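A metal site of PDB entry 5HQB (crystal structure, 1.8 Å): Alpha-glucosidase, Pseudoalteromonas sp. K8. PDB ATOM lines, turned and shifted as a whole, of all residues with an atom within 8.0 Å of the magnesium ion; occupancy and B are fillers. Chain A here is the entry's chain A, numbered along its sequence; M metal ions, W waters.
The side-chain carboxylate (OD1) of Asp 592 is in hydrogen-bond range of the side-chain hydroxyl (OG1) of Thr 591 (3.3 Å).
The backbone carbonyl oxygen of Asp 566 lies close to the side-chain hydroxyl of Thr 591.
The side-chain carboxylate (OD1) of Asp 592 is in hydrogen-bond range of the backbone NH (N) of Gln 594.
The side-chain carboxylate of Asp 592 lies within salt-bridge range of the guanidinium group of Arg 596.
The backbone NH (N) of Asp 566 lies within hydrogen-bond range of the side-chain hydroxyl (OG) of Ser 476, at 3.2 Å.
The backbone NH of Gly 565 sits at hydrogen-bond distance from the backbone carbonyl oxygen of Ser 476 (2.9 Å).
The guanidinium group (NH2) of Arg 596 is in salt-bridge range of the side-chain carboxylate (OD1) of Asp 566 (3.9 Å).
Three residues have an atom within 4 Å of the magnesium ion: Gly 565, Asp 566 and Asp 592.
Along chain A the residues within 4 Å of the magnesium ion span positions 565 to 592.
The magnesium ion is bound by OD2 of Asp 592 (2.0 Å), water W1 (2.0 Å), O of Gly 565 (2.0 Å), OD2 of Asp 566 (2.1 Å), water W3 (2.1 Å) and water W2 (2.2 Å).
The magnesium ion has six donor atoms within binding distance.
Water W1 lies within hydrogen-bond range of the side-chain carboxylate (OE1) of Glu 473 and the side-chain carboxylate (OE1) of Glu 593.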
ATOM      1  N   TRP A 143      22.434   0.289  27.399  1.00  0.00           N
ATOM      2  CA  TRP A 143      20.999   0.491  27.199  1.00  0.00           C
ATOM      3  C   TRP A 143      20.512   1.407  28.317  1.00  0.00           C
ATOM      4  O   TRP A 143      20.479   0.990  29.486  1.00  0.00           O
ATOM      5  CB  TRP A 143      20.247  -0.836  27.212  1.00  0.00           C
ATOM      6  CG  TRP A 143      20.801  -1.882  26.271  1.00  0.00           C
ATOM      7  CD1 TRP A 143      20.498  -2.029  24.945  1.00  0.00           C
ATOM      8  CD2 TRP A 143      21.734  -2.918  26.594  1.00  0.00           C
ATOM      9  NE1 TRP A 143      21.191  -3.099  24.429  1.00  0.00           N
ATOM     10  CE2 TRP A 143      21.950  -3.665  25.422  1.00  0.00           C
ATOM     11  CE3 TRP A 143      22.396  -3.284  27.776  1.00  0.00           C
ATOM     12  CZ2 TRP A 143      22.815  -4.762  25.378  1.00  0.00           C
ATOM     13  CZ3 TRP A 143      23.261  -4.382  27.732  1.00  0.00           C
ATOM     14  CH2 TRP A 143      23.455  -5.114  26.541  1.00  0.00           C
ATOM     15  N   THR A 159      20.009   2.515  22.740  1.00  0.00           N
ATOM     16  CA  THR A 159      21.001   1.453  22.555  1.00  0.00           C
ATOM     17  C   THR A 159      22.206   2.095  21.880  1.00  0.00           C
ATOM     18  O   THR A 159      22.126   2.485  20.707  1.00  0.00           O
ATOM     19  CB  THR A 159      20.449   0.314  21.687  1.00  0.00           C
ATOM     20  OG1 THR A 159      19.231  -0.187  22.257  1.00  0.00           O
ATOM     21  CG2 THR A 159      21.467  -0.828  21.570  1.00  0.00           C
ATOM     22  N   PRO A 472       8.139  -1.688  20.206  1.00  0.00           N
ATOM     23  CA  PRO A 472       8.094  -3.120  20.508  1.00  0.00           C
ATOM     24  C   PRO A 472       9.169  -3.597  21.484  1.00  0.00           C
ATOM     25  O   PRO A 472       8.904  -4.498  22.295  1.00  0.00           O
ATOM     26  CB  PRO A 472       8.259  -3.765  19.129  1.00  0.00           C
ATOM     27  CG  PRO A 472       7.548  -2.771  18.197  1.00  0.00           C
ATOM     28  CD  PRO A 472       7.903  -1.404  18.766  1.00  0.00           C
ATOM     29  N   GLU A 473      10.378  -3.028  21.430  1.00  0.00           N
ATOM     30  CA  GLU A 473      11.464  -3.488  22.292  1.00  0.00           C
ATOM     31  C   GLU A 473      11.318  -3.039  23.738  1.00  0.00           C
ATOM     32  O   GLU A 473      12.109  -3.460  24.588  1.00  0.00           O
ATOM     33  CB  GLU A 473      12.820  -2.998  21.734  1.00  0.00           C
ATOM     34  CG  GLU A 473      13.035  -1.493  21.916  1.00  0.00           C
ATOM     35  CD  GLU A 473      14.377  -1.016  21.343  1.00  0.00           C
ATOM     36  OE1 GLU A 473      15.129  -1.839  20.773  1.00  0.00           O
ATOM     37  OE2 GLU A 473      14.663   0.197  21.460  1.00  0.00           O
ATOM     38  N   HIS A 474      10.314  -2.209  24.047  1.00  0.00           N
ATOM     39  CA  HIS A 474      10.309  -1.504  25.339  1.00  0.00           C
ATOM     40  C   HIS A 474      10.288  -2.475  26.517  1.00  0.00           C
ATOM     41  O   HIS A 474      11.036  -2.299  27.485  1.00  0.00           O
ATOM     42  CB  HIS A 474       9.111  -0.531  25.410  1.00  0.00           C
ATOM     43  CG  HIS A 474       9.109   0.319  26.640  1.00  0.00           C
ATOM     44  ND1 HIS A 474      10.155   1.162  26.966  1.00  0.00           N
ATOM     45  CD2 HIS A 474       8.187   0.467  27.620  1.00  0.00           C
ATOM     46  CE1 HIS A 474       9.880   1.786  28.095  1.00  0.00           C
ATOM     47  NE2 HIS A 474       8.693   1.376  28.519  1.00  0.00           N
ATOM     48  N   SER A 476      11.320  -5.570  26.724  1.00  0.00           N
ATOM     49  CA  SER A 476      12.583  -6.273  26.817  1.00  0.00           C
ATOM     50  C   SER A 476      13.735  -5.345  27.194  1.00  0.00           C
ATOM     51  O   SER A 476      14.808  -5.843  27.545  1.00  0.00           O
ATOM     52  CB  SER A 476      12.900  -6.977  25.490  1.00  0.00           C
ATOM     53  OG  SER A 476      13.211  -6.019  24.493  1.00  0.00           O
ATOM     54  N   MET A 477      13.541  -4.026  27.117  1.00  0.00           N
ATOM     55  CA  MET A 477      14.458  -3.089  27.752  1.00  0.00           C
ATOM     56  C   MET A 477      14.178  -2.976  29.248  1.00  0.00           C
ATOM     57  O   MET A 477      15.084  -3.116  30.069  1.00  0.00           O
ATOM     58  CB  MET A 477      14.346  -1.706  27.103  1.00  0.00           C
ATOM     59  CG  MET A 477      14.828  -1.665  25.672  1.00  0.00           C
ATOM     60  SD  MET A 477      16.627  -1.913  25.572  1.00  0.00           S
ATOM     61  CE  MET A 477      16.851  -1.696  23.806  1.00  0.00           C
ATOM     62  N   ALA A 563      17.719 -11.552  26.514  1.00  0.00           N
ATOM     63  CA  ALA A 563      18.782 -10.685  26.026  1.00  0.00           C
ATOM     64  C   ALA A 563      18.257  -9.253  26.048  1.00  0.00           C
ATOM     65  O   ALA A 563      17.100  -9.023  25.670  1.00  0.00           O
ATOM     66  CB  ALA A 563      19.235 -11.109  24.623  1.00  0.00           C
ATOM     67  N   VAL A 564      19.081  -8.312  26.511  1.00  0.00           N
ATOM     68  CA  VAL A 564      18.581  -6.951  26.723  1.00  0.00           C
ATOM     69  C   VAL A 564      18.083  -6.368  25.408  1.00  0.00           C
ATOM     70  O   VAL A 564      18.801  -6.387  24.396  1.00  0.00           O
ATOM     71  CB  VAL A 564      19.662  -6.048  27.313  1.00  0.00           C
ATOM     72  CG1 VAL A 564      19.039  -4.694  27.650  1.00  0.00           C
ATOM     73  CG2 VAL A 564      20.335  -6.704  28.548  1.00  0.00           C
ATOM     74  N   GLY A 565      16.858  -5.839  25.438  1.00  0.00           N
ATOM     75  CA  GLY A 565      16.274  -5.227  24.260  1.00  0.00           C
ATOM     76  C   GLY A 565      15.834  -6.202  23.189  1.00  0.00           C
ATOM     77  O   GLY A 565      15.466  -5.769  22.084  1.00  0.00           O
ATOM     78  N   ASP A 566      15.850  -7.510  23.474  1.00  0.00           N
ATOM     79  CA  ASP A 566      15.420  -8.526  22.519  1.00  0.00           C
ATOM     80  C   ASP A 566      14.304  -9.396  23.080  1.00  0.00           C
ATOM     81  O   ASP A 566      13.266  -9.505  22.432  1.00  0.00           O
ATOM     82  CB  ASP A 566      16.608  -9.405  22.093  1.00  0.00           C
ATOM     83  CG  ASP A 566      17.605  -8.662  21.205  1.00  0.00           C
ATOM     84  OD1 ASP A 566      18.732  -9.166  21.014  1.00  0.00           O
ATOM     85  OD2 ASP A 566      17.269  -7.565  20.708  1.00  0.00           O
ATOM     86  N   PHE A 567      14.493 -10.045  24.236  1.00  0.00           N
ATOM     87  CA  PHE A 567      13.429 -10.926  24.743  1.00  0.00           C
ATOM     88  C   PHE A 567      13.731 -11.279  26.198  1.00  0.00           C
ATOM     89  O   PHE A 567      14.848 -11.102  26.688  1.00  0.00           O
ATOM     90  CB  PHE A 567      13.295 -12.200  23.892  1.00  0.00           C
ATOM     91  CG  PHE A 567      14.409 -13.196  24.092  1.00  0.00           C
ATOM     92  CD1 PHE A 567      15.634 -13.021  23.468  1.00  0.00           C
ATOM     93  CD2 PHE A 567      14.209 -14.340  24.869  1.00  0.00           C
ATOM     94  CE1 PHE A 567      16.670 -13.951  23.655  1.00  0.00           C
ATOM     95  CE2 PHE A 567      15.221 -15.274  25.048  1.00  0.00           C
ATOM     96  CZ  PHE A 567      16.452 -15.082  24.437  1.00  0.00           C
ATOM     97  N   THR A 591       8.921 -10.669  23.231  1.00  0.00           N
ATOM     98  CA  THR A 591       9.992 -10.322  22.305  1.00  0.00           C
ATOM     99  C   THR A 591       9.912  -8.842  21.957  1.00  0.00           C
ATOM    100  O   THR A 591       9.016  -8.118  22.416  1.00  0.00           O
ATOM    101  CB  THR A 591       9.930 -11.202  21.048  1.00  0.00           C
ATOM    102  OG1 THR A 591      11.064 -10.912  20.222  1.00  0.00           O
ATOM    103  CG2 THR A 591       8.644 -10.918  20.262  1.00  0.00           C
ATOM    104  N   ASP A 592      10.867  -8.393  21.150  1.00  0.00           N
ATOM    105  CA  ASP A 592      10.929  -7.012  20.669  1.00  0.00           C
ATOM    106  C   ASP A 592      10.241  -6.916  19.298  1.00  0.00           C
ATOM    107  O   ASP A 592       9.251  -7.614  19.071  1.00  0.00           O
ATOM    108  CB  ASP A 592      12.390  -6.538  20.602  1.00  0.00           C
ATOM    109  CG  ASP A 592      13.276  -7.436  19.736  1.00  0.00           C
ATOM    110  OD1 ASP A 592      12.748  -8.363  19.091  1.00  0.00           O
ATOM    111  OD2 ASP A 592      14.507  -7.195  19.663  1.00  0.00           O
ATOM    112  N   GLU A 593      10.770  -6.102  18.387  1.00  0.00           N
ATOM    113  CA  GLU A 593      10.152  -5.978  17.066  1.00  0.00           C
ATOM    114  C   GLU A 593      10.299  -7.232  16.204  1.00  0.00           C
ATOM    115  O   GLU A 593       9.601  -7.348  15.187  1.00  0.00           O
ATOM    116  CB  GLU A 593      10.739  -4.772  16.296  1.00  0.00           C
ATOM    117  CG  GLU A 593      12.157  -4.978  15.735  1.00  0.00           C
ATOM    118  CD  GLU A 593      13.250  -4.877  16.815  1.00  0.00           C
ATOM    119  OE1 GLU A 593      12.940  -4.423  17.952  1.00  0.00           O
ATOM    120  OE2 GLU A 593      14.405  -5.248  16.522  1.00  0.00           O
ATOM    121  N   GLN A 594      11.165  -8.165  16.585  1.00  0.00           N
ATOM    122  CA  GLN A 594      11.414  -9.361  15.789  1.00  0.00           C
ATOM    123  C   GLN A 594      10.584 -10.534  16.306  1.00  0.00           C
ATOM    124  O   GLN A 594      10.455 -10.721  17.519  1.00  0.00           O
ATOM    125  CB  GLN A 594      12.898  -9.759  15.823  1.00  0.00           C
ATOM    126  CG  GLN A 594      13.842  -8.736  15.192  1.00  0.00           C
ATOM    127  CD  GLN A 594      15.250  -9.292  14.997  1.00  0.00           C
ATOM    128  OE1 GLN A 594      15.490 -10.492  15.164  1.00  0.00           O
ATOM    129  NE2 GLN A 594      16.178  -8.418  14.627  1.00  0.00           N
ATOM    130  N   ARG A 596      10.477 -14.321  17.238  1.00  0.00           N
ATOM    131  CA  ARG A 596      11.566 -15.111  17.817  1.00  0.00           C
ATOM    132  C   ARG A 596      11.060 -16.483  18.240  1.00  0.00           C
ATOM    133  O   ARG A 596       9.955 -16.607  18.784  1.00  0.00           O
ATOM    134  CB  ARG A 596      12.222 -14.402  19.034  1.00  0.00           C
ATOM    135  CG  ARG A 596      12.940 -13.072  18.730  1.00  0.00           C
ATOM    136  CD  ARG A 596      13.680 -12.440  19.966  1.00  0.00           C
ATOM    137  NE  ARG A 596      14.181 -11.110  19.579  1.00  0.00           N
ATOM    138  CZ  ARG A 596      15.321 -10.916  18.924  1.00  0.00           C
ATOM    139  NH1 ARG A 596      16.091 -11.952  18.628  1.00  0.00           N
ATOM    140  NH2 ARG A 596      15.690  -9.686  18.565  1.00  0.00           N
HETATM  141 MG    MG M   1      16.051  -5.958  20.134  1.00  0.00          MG
HETATM  142  O   HOH W   1      15.105  -4.226  19.604  1.00  0.00           O
HETATM  143  O   HOH W   2      17.746  -4.671  20.535  1.00  0.00           O
HETATM  144  O   HOH W   3      16.602  -6.140  18.100  1.00  0.00           O
